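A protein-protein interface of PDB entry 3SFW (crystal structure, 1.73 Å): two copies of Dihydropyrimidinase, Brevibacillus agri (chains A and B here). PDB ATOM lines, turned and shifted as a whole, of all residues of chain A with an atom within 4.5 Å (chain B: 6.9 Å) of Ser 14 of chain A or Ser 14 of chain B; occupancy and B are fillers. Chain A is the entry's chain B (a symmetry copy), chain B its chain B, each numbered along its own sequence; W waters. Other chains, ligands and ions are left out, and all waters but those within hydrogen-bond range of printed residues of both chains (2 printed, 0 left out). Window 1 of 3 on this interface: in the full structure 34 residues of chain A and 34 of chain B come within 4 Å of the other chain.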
ATOM      1  N   THR A  12     -22.539  -9.866 -13.429  1.00  0.00           N
ATOM      2  CA  THR A  12     -22.090 -11.061 -12.720  1.00  0.00           C
ATOM      3  C   THR A  12     -22.207 -10.812 -11.211  1.00  0.00           C
ATOM      4  O   THR A  12     -22.856  -9.872 -10.801  1.00  0.00           O
ATOM      5  CB  THR A  12     -20.652 -11.465 -13.088  1.00  0.00           C
ATOM      6  OG1 THR A  12     -19.735 -10.471 -12.608  1.00  0.00           O
ATOM      7  CG2 THR A  12     -20.501 -11.621 -14.660  1.00  0.00           C
ATOM      8  N   ALA A  13     -21.623 -11.689 -10.393  1.00  0.00           N
ATOM      9  CA  ALA A  13     -21.699 -11.480  -8.948  1.00  0.00           C
ATOM     10  C   ALA A  13     -20.843 -10.300  -8.483  1.00  0.00           C
ATOM     11  O   ALA A  13     -21.079  -9.766  -7.387  1.00  0.00           O
ATOM     12  CB  ALA A  13     -21.325 -12.763  -8.197  1.00  0.00           C
ATOM     13  N   SER A  14     -19.869  -9.877  -9.312  1.00  0.00           N
ATOM     14  CA  SER A  14     -19.026  -8.723  -8.992  1.00  0.00           C
ATOM     15  C   SER A  14     -19.228  -7.534  -9.915  1.00  0.00           C
ATOM     16  O   SER A  14     -19.260  -6.392  -9.459  1.00  0.00           O
ATOM     17  CB  SER A  14     -17.532  -9.081  -8.943  1.00  0.00           C
ATOM     18  OG  SER A  14     -17.086  -9.768 -10.115  1.00  0.00           O
ATOM     19  N   ASP A  15     -19.422  -7.812 -11.210  1.00  0.00           N
ATOM     20  CA  ASP A  15     -19.223  -6.829 -12.304  1.00  0.00           C
ATOM     21  C   ASP A  15     -20.554  -6.425 -12.982  1.00  0.00           C
ATOM     22  O   ASP A  15     -21.481  -7.237 -13.055  1.00  0.00           O
ATOM     23  CB  ASP A  15     -18.272  -7.421 -13.385  1.00  0.00           C
ATOM     24  CG  ASP A  15     -16.828  -7.616 -12.856  1.00  0.00           C
ATOM     25  OD1 ASP A  15     -16.270  -6.644 -12.331  1.00  0.00           O
ATOM     26  OD2 ASP A  15     -16.303  -8.753 -12.883  1.00  0.00           O
ATOM     27  N   THR A  16     -20.656  -5.169 -13.426  1.00  0.00           N
ATOM     28  CA  THR A  16     -21.776  -4.738 -14.302  1.00  0.00           C
ATOM     29  C   THR A  16     -21.210  -3.785 -15.348  1.00  0.00           C
ATOM     30  O   THR A  16     -20.608  -2.773 -15.006  1.00  0.00           O
ATOM     31  CB  THR A  16     -22.906  -4.001 -13.519  1.00  0.00           C
ATOM     32  OG1 THR A  16     -23.364  -4.839 -12.453  1.00  0.00           O
ATOM     33  CG2 THR A  16     -24.126  -3.683 -14.453  1.00  0.00           C
ATOM     34  N   ASN A 362     -25.972  -7.338  -8.408  1.00  0.00           N
ATOM     35  CA  ASN A 362     -24.861  -8.302  -8.330  1.00  0.00           C
ATOM     36  C   ASN A 362     -25.104  -9.397  -7.289  1.00  0.00           C
ATOM     37  O   ASN A 362     -24.810 -10.557  -7.531  1.00  0.00           O
ATOM     38  CB  ASN A 362     -23.520  -7.594  -8.042  1.00  0.00           C
ATOM     39  CG  ASN A 362     -23.105  -6.623  -9.160  1.00  0.00           C
ATOM     40  OD1 ASN A 362     -22.896  -7.013 -10.337  1.00  0.00           O
ATOM     41  ND2 ASN A 362     -23.027  -5.357  -8.811  1.00  0.00           N
ATOM     42  N   LYS A 374     -20.257 -22.287  -6.578  1.00  0.00           N
ATOM     43  CA  LYS A 374     -19.099 -22.393  -5.678  1.00  0.00           C
ATOM     44  C   LYS A 374     -19.347 -23.381  -4.538  1.00  0.00           C
ATOM     45  O   LYS A 374     -18.492 -24.195  -4.234  1.00  0.00           O
ATOM     46  CB  LYS A 374     -18.718 -21.019  -5.137  1.00  0.00           C
ATOM     47  CG  LYS A 374     -18.136 -20.116  -6.269  1.00  0.00           C
ATOM     48  CD  LYS A 374     -17.834 -18.729  -5.809  1.00  0.00           C
ATOM     49  CE  LYS A 374     -16.823 -18.085  -6.785  1.00  0.00           C
ATOM     50  NZ  LYS A 374     -16.720 -16.633  -6.554  1.00  0.00           N
ATOM     51  N   PHE A 379     -18.037 -24.619 -10.050  1.00  0.00           N
ATOM     52  CA  PHE A 379     -17.377 -23.374 -10.448  1.00  0.00           C
ATOM     53  C   PHE A 379     -15.894 -23.656 -10.780  1.00  0.00           C
ATOM     54  O   PHE A 379     -15.209 -24.338 -10.020  1.00  0.00           O
ATOM     55  CB  PHE A 379     -17.443 -22.360  -9.303  1.00  0.00           C
ATOM     56  CG  PHE A 379     -17.044 -20.988  -9.699  1.00  0.00           C
ATOM     57  CD1 PHE A 379     -15.745 -20.544  -9.494  1.00  0.00           C
ATOM     58  CD2 PHE A 379     -17.971 -20.122 -10.278  1.00  0.00           C
ATOM     59  CE1 PHE A 379     -15.372 -19.257  -9.900  1.00  0.00           C
ATOM     60  CE2 PHE A 379     -17.599 -18.835 -10.668  1.00  0.00           C
ATOM     61  CZ  PHE A 379     -16.307 -18.411 -10.488  1.00  0.00           C
ATOM     62  N   VAL B  11      -7.894 -12.803 -11.468  1.00  0.00           N
ATOM     63  CA  VAL B  11      -8.673 -13.088 -10.252  1.00  0.00           C
ATOM     64  C   VAL B  11      -9.457 -11.840  -9.891  1.00  0.00           C
ATOM     65  O   VAL B  11      -8.886 -10.760  -9.795  1.00  0.00           O
ATOM     66  CB  VAL B  11      -7.751 -13.465  -9.072  1.00  0.00           C
ATOM     67  CG1 VAL B  11      -8.600 -13.924  -7.851  1.00  0.00           C
ATOM     68  CG2 VAL B  11      -6.794 -14.580  -9.503  1.00  0.00           C
ATOM     69  N   THR B  12     -10.778 -11.972  -9.756  1.00  0.00           N
ATOM     70  CA  THR B  12     -11.599 -10.850  -9.311  1.00  0.00           C
ATOM     71  C   THR B  12     -12.377 -11.274  -8.059  1.00  0.00           C
ATOM     72  O   THR B  12     -12.054 -12.279  -7.458  1.00  0.00           O
ATOM     73  CB  THR B  12     -12.566 -10.354 -10.400  1.00  0.00           C
ATOM     74  OG1 THR B  12     -13.553 -11.362 -10.664  1.00  0.00           O
ATOM     75  CG2 THR B  12     -11.777 -10.013 -11.734  1.00  0.00           C
ATOM     76  N   ALA B  13     -13.360 -10.476  -7.642  1.00  0.00           N
ATOM     77  CA  ALA B  13     -14.134 -10.852  -6.460  1.00  0.00           C
ATOM     78  C   ALA B  13     -15.057 -12.045  -6.721  1.00  0.00           C
ATOM     79  O   ALA B  13     -15.485 -12.709  -5.763  1.00  0.00           O
ATOM     80  CB  ALA B  13     -14.924  -9.649  -5.928  1.00  0.00           C
ATOM     81  N   SER B  14     -15.347 -12.334  -8.004  1.00  0.00           N
ATOM     82  CA  SER B  14     -16.175 -13.484  -8.371  1.00  0.00           C
ATOM     83  C   SER B  14     -15.428 -14.567  -9.131  1.00  0.00           C
ATOM     84  O   SER B  14     -15.626 -15.753  -8.877  1.00  0.00           O
ATOM     85  CB  SER B  14     -17.428 -13.079  -9.163  1.00  0.00           C
ATOM     86  OG  SER B  14     -17.131 -12.246 -10.287  1.00  0.00           O
ATOM     87  N   ASP B  15     -14.524 -14.149 -10.027  1.00  0.00           N
ATOM     88  CA  ASP B  15     -14.011 -14.992 -11.135  1.00  0.00           C
ATOM     89  C   ASP B  15     -12.521 -15.365 -10.949  1.00  0.00           C
ATOM     90  O   ASP B  15     -11.756 -14.585 -10.374  1.00  0.00           O
ATOM     91  CB  ASP B  15     -14.174 -14.246 -12.491  1.00  0.00           C
ATOM     92  CG  ASP B  15     -15.661 -14.059 -12.887  1.00  0.00           C
ATOM     93  OD1 ASP B  15     -16.383 -15.064 -12.901  1.00  0.00           O
ATOM     94  OD2 ASP B  15     -16.112 -12.908 -13.085  1.00  0.00           O
ATOM     95  N   THR B  16     -12.132 -16.566 -11.390  1.00  0.00           N
ATOM     96  CA  THR B  16     -10.696 -16.935 -11.490  1.00  0.00           C
ATOM     97  C   THR B  16     -10.509 -17.740 -12.771  1.00  0.00           C
ATOM     98  O   THR B  16     -11.159 -18.762 -12.963  1.00  0.00           O
ATOM     99  CB  THR B  16     -10.210 -17.797 -10.285  1.00  0.00           C
ATOM    100  OG1 THR B  16     -10.491 -17.105  -9.065  1.00  0.00           O
ATOM    101  CG2 THR B  16      -8.663 -18.052 -10.361  1.00  0.00           C
ATOM    102  N   ASN B 362     -10.830 -15.183  -4.005  1.00  0.00           N
ATOM    103  CA  ASN B 362     -11.813 -14.194  -4.480  1.00  0.00           C
ATOM    104  C   ASN B 362     -12.264 -13.236  -3.377  1.00  0.00           C
ATOM    105  O   ASN B 362     -12.404 -12.046  -3.610  1.00  0.00           O
ATOM    106  CB  ASN B 362     -13.042 -14.880  -5.114  1.00  0.00           C
ATOM    107  CG  ASN B 362     -12.690 -15.701  -6.366  1.00  0.00           C
ATOM    108  OD1 ASN B 362     -12.187 -15.171  -7.389  1.00  0.00           O
ATOM    109  ND2 ASN B 362     -12.910 -16.995  -6.275  1.00  0.00           N
ATOM    110  N   GLN B 363     -12.393 -13.732  -2.148  1.00  0.00           N
ATOM    111  CA  GLN B 363     -12.696 -12.831  -1.029  1.00  0.00           C
ATOM    112  C   GLN B 363     -11.585 -11.846  -0.775  1.00  0.00           C
ATOM    113  O   GLN B 363     -11.842 -10.726  -0.374  1.00  0.00           O
ATOM    114  CB  GLN B 363     -12.954 -13.612   0.268  1.00  0.00           C
ATOM    115  CG  GLN B 363     -14.221 -14.428   0.229  1.00  0.00           C
ATOM    116  CD  GLN B 363     -14.450 -15.147   1.551  1.00  0.00           C
ATOM    117  OE1 GLN B 363     -13.549 -15.808   2.061  1.00  0.00           O
ATOM    118  NE2 GLN B 363     -15.623 -14.909   2.176  1.00  0.00           N
ATOM    119  N   VAL B 365      -9.708 -10.462  -3.020  1.00  0.00           N
ATOM    120  CA  VAL B 365      -9.872  -9.334  -3.916  1.00  0.00           C
ATOM    121  C   VAL B 365     -11.042  -8.463  -3.498  1.00  0.00           C
ATOM    122  O   VAL B 365     -10.957  -7.240  -3.543  1.00  0.00           O
ATOM    123  CB  VAL B 365     -10.069  -9.819  -5.390  1.00  0.00           C
ATOM    124  CG1 VAL B 365     -10.489  -8.640  -6.276  1.00  0.00           C
ATOM    125  CG2 VAL B 365      -8.777 -10.425  -5.882  1.00  0.00           C
ATOM    126  N   ASP B 366     -12.173  -9.083  -3.143  1.00  0.00           N
ATOM    127  CA  ASP B 366     -13.332  -8.302  -2.669  1.00  0.00           C
ATOM    128  C   ASP B 366     -12.972  -7.359  -1.514  1.00  0.00           C
ATOM    129  O   ASP B 366     -13.351  -6.192  -1.491  1.00  0.00           O
ATOM    130  CB  ASP B 366     -14.458  -9.259  -2.224  1.00  0.00           C
ATOM    131  CG  ASP B 366     -15.852  -8.706  -2.511  1.00  0.00           C
ATOM    132  OD1 ASP B 366     -16.013  -7.672  -3.198  1.00  0.00           O
ATOM    133  OD2 ASP B 366     -16.803  -9.268  -1.944  1.00  0.00           O
ATOM    134  N   THR B 370     -12.638  -4.643  -4.552  1.00  0.00           N
ATOM    135  CA  THR B 370     -13.961  -4.519  -5.162  1.00  0.00           C
ATOM    136  C   THR B 370     -15.024  -3.938  -4.200  1.00  0.00           C
ATOM    137  O   THR B 370     -15.765  -2.996  -4.540  1.00  0.00           O
ATOM    138  CB  THR B 370     -14.428  -5.861  -5.734  1.00  0.00           C
ATOM    139  OG1 THR B 370     -13.369  -6.442  -6.528  1.00  0.00           O
ATOM    140  CG2 THR B 370     -15.698  -5.667  -6.608  1.00  0.00           C
ATOM    141  N   LYS B 374     -17.087  -0.341  -4.160  1.00  0.00           N
ATOM    142  CA  LYS B 374     -18.556  -0.295  -4.100  1.00  0.00           C
ATOM    143  C   LYS B 374     -19.057   0.545  -2.926  1.00  0.00           C
ATOM    144  O   LYS B 374     -19.959   1.351  -3.087  1.00  0.00           O
ATOM    145  CB  LYS B 374     -19.130  -1.707  -4.045  1.00  0.00           C
ATOM    146  CG  LYS B 374     -18.908  -2.453  -5.398  1.00  0.00           C
ATOM    147  CD  LYS B 374     -19.370  -3.871  -5.363  1.00  0.00           C
ATOM    148  CE  LYS B 374     -19.597  -4.362  -6.812  1.00  0.00           C
ATOM    149  NZ  LYS B 374     -19.761  -5.825  -6.852  1.00  0.00           N
ATOM    150  N   PHE B 379     -16.948   2.454  -7.979  1.00  0.00           N
ATOM    151  CA  PHE B 379     -17.205   1.288  -8.827  1.00  0.00           C
ATOM    152  C   PHE B 379     -18.224   1.661  -9.927  1.00  0.00           C
ATOM    153  O   PHE B 379     -19.248   2.277  -9.639  1.00  0.00           O
ATOM    154  CB  PHE B 379     -17.782   0.148  -7.984  1.00  0.00           C
ATOM    155  CG  PHE B 379     -17.823  -1.154  -8.693  1.00  0.00           C
ATOM    156  CD1 PHE B 379     -18.980  -1.570  -9.337  1.00  0.00           C
ATOM    157  CD2 PHE B 379     -16.701  -1.981  -8.716  1.00  0.00           C
ATOM    158  CE1 PHE B 379     -18.998  -2.787 -10.029  1.00  0.00           C
ATOM    159  CE2 PHE B 379     -16.728  -3.201  -9.394  1.00  0.00           C
ATOM    160  CZ  PHE B 379     -17.865  -3.595 -10.052  1.00  0.00           C
ATOM    161  N   GLY B 383     -11.718  -1.004  -8.908  1.00  0.00           N
ATOM    162  CA  GLY B 383     -12.048  -2.137  -8.022  1.00  0.00           C
ATOM    163  C   GLY B 383     -12.298  -3.459  -8.720  1.00  0.00           C
ATOM    164  O   GLY B 383     -12.611  -4.469  -8.075  1.00  0.00           O
ATOM    165  N   THR B 384     -12.089  -3.523 -10.039  1.00  0.00           N
ATOM    166  CA  THR B 384     -12.241  -4.807 -10.695  1.00  0.00           C
ATOM    167  C   THR B 384     -11.378  -4.956 -11.969  1.00  0.00           C
ATOM    168  O   THR B 384     -10.652  -4.043 -12.350  1.00  0.00           O
ATOM    169  CB  THR B 384     -13.737  -5.103 -11.042  1.00  0.00           C
ATOM    170  OG1 THR B 384     -13.894  -6.497 -11.344  1.00  0.00           O
ATOM    171  CG2 THR B 384     -14.232  -4.241 -12.237  1.00  0.00           C
HETATM  172  O   HOH W   1     -14.658 -10.515 -12.953  1.00  0.00           O
HETATM  173  O   HOH W   2     -17.471 -11.090 -13.899  1.00  0.00           O
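The side-chain carboxylate (OD1) of Asp 15 of chain A lies within hydrogen-bond range of the side-chain hydroxyl (OG1) of Thr 384 of chain B (2.6 Å).
O of Ser 14 of chain A is in hydrogen-bond range of NZ of Lys 374 of chain B.
O of Ser 14 of chain B lies within hydrogen-bond range of NZ of Lys 374 of chain A, 2.7 Å away.
The side-chain hydroxyl (OG) of Ser 14 of chain A sits at hydrogen-bond distance from the side-chain hydroxyl (OG) of Ser 14 of chain B (2.5 Å).
The side-chain hydroxyl (OG1) of Thr 12 of chain B lies within hydrogen-bond range of the backbone NH (N) of Asp 15 of chain B (3.0 Å).
OG1 of Thr 12 of chain A sits close to N of Ser 14 of chain A.
The backbone NH (N) of Ser 14 of chain B sits close to the side-chain hydroxyl (OG1) of Thr 12 of chain B, at 3.4 Å.
O of Thr 12 of chain A sits close to OD1 of Asn 362 of chain A (2.9 Å).
OD2 of Asp 15 of chain A lies within hydrogen-bond range of OG of Ser 14 of chain A (3.1 Å).
OD1 of Asn 362 of chain B sits close to O of Thr 12 of chain B (2.9 Å).
Among the printed residues, merely in contact across the chains: Ser 14 of chain A with Phe 379 of chain B (3.2 Å), Phe 379 of chain A with Ser 14 of chain B (3.2 Å), Asn 362 of chain A with Lys 374 of chain B (3.8 Å), Lys 374 of chain A with Asn 362 of chain B (3.8 Å), Thr 12 of chain A with Ser 14 of chain B (3.9 Å) and Ser 14 of chain A with Thr 12 of chain B (3.9 Å).
Ser 14 of chain B touches just these residues of chain A: Thr 12, Ser 14, Lys 374 and Phe 379.
Of the printed residues of chain B, Lys 374 of chain A touches Ser 14 (2.7 Å) and Asn 362 (3.8 Å).
Of the printed residues of chain A, Phe 379 of chain B touches Ser 14.
Of the printed residues of chain A, Lys 374 of chain B touches Ser 14 (2.7 Å) and Asn 362 (3.8 Å).
Of the printed residues of chain A, Thr 384 of chain B touches Asp 15.
Of the printed residues of chain B, Asn 362 of chain A touches Lys 374 (3.8 Å).
Thr 370 of chain B touches none of the printed residues of chain A.
Thr 16 of chain B touches none of the printed residues of chain A.
The nearest residue of chain B that does not touch Ser 14 of chain A is Ala 13 of chain B (4.03 Å).
The nearest printed residue of chain B that does not touch Lys 374 of chain A is Ala 13 of chain B (4.2 Å).
Of the 8 printed residues of chain A, 6 touch a printed residue of chain B.
Along chain A the printed residues that touch a printed residue of chain B span positions 12 to 379.
Hydrophobic or aromatic side chains of chain B within 4 Å of the printed part of chain A: Phe 379.
Thr 12 of chain A touches Ser 14 of chain B, and with the chains exchanged Ser 14 of chain A touches Thr 12 of chain B.
Ser 14 of chain A touches its own counterpart, Ser 14 of chain B.
Ser 14 of chain A touches Lys 374 of chain B, and with the chains exchanged Lys 374 of chain A touches Ser 14 of chain B.
Ser 14 of chain A touches Phe 379 of chain B, and with the chains exchanged Phe 379 of chain A touches Ser 14 of chain B.
Positions printed for both chains: 12, 13, 14, 15, 16, 362, 374 and 379.
Of the 10 pairs that touch across the chains among the printed residues, 9 have their exchanged pair printed and touching as well.
Water W1 lies within hydrogen-bond range of the side-chain carboxylate (OD2) of Asp 15 of chain A (2.4 Å), the side-chain hydroxyl (OG1) of Thr 12 of chain B (2.7 Å) and the side-chain carboxylate (OD2) of Asp 15 of chain B (2.8 Å).
Water W2 lies within hydrogen-bond range of the side-chain carboxylate (OD2) of Asp 15 of chain B, the side-chain hydroxyl (OG1) of Thr 12 of chain A and the side-chain carboxylate (OD2) of Asp 15 of chain A.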
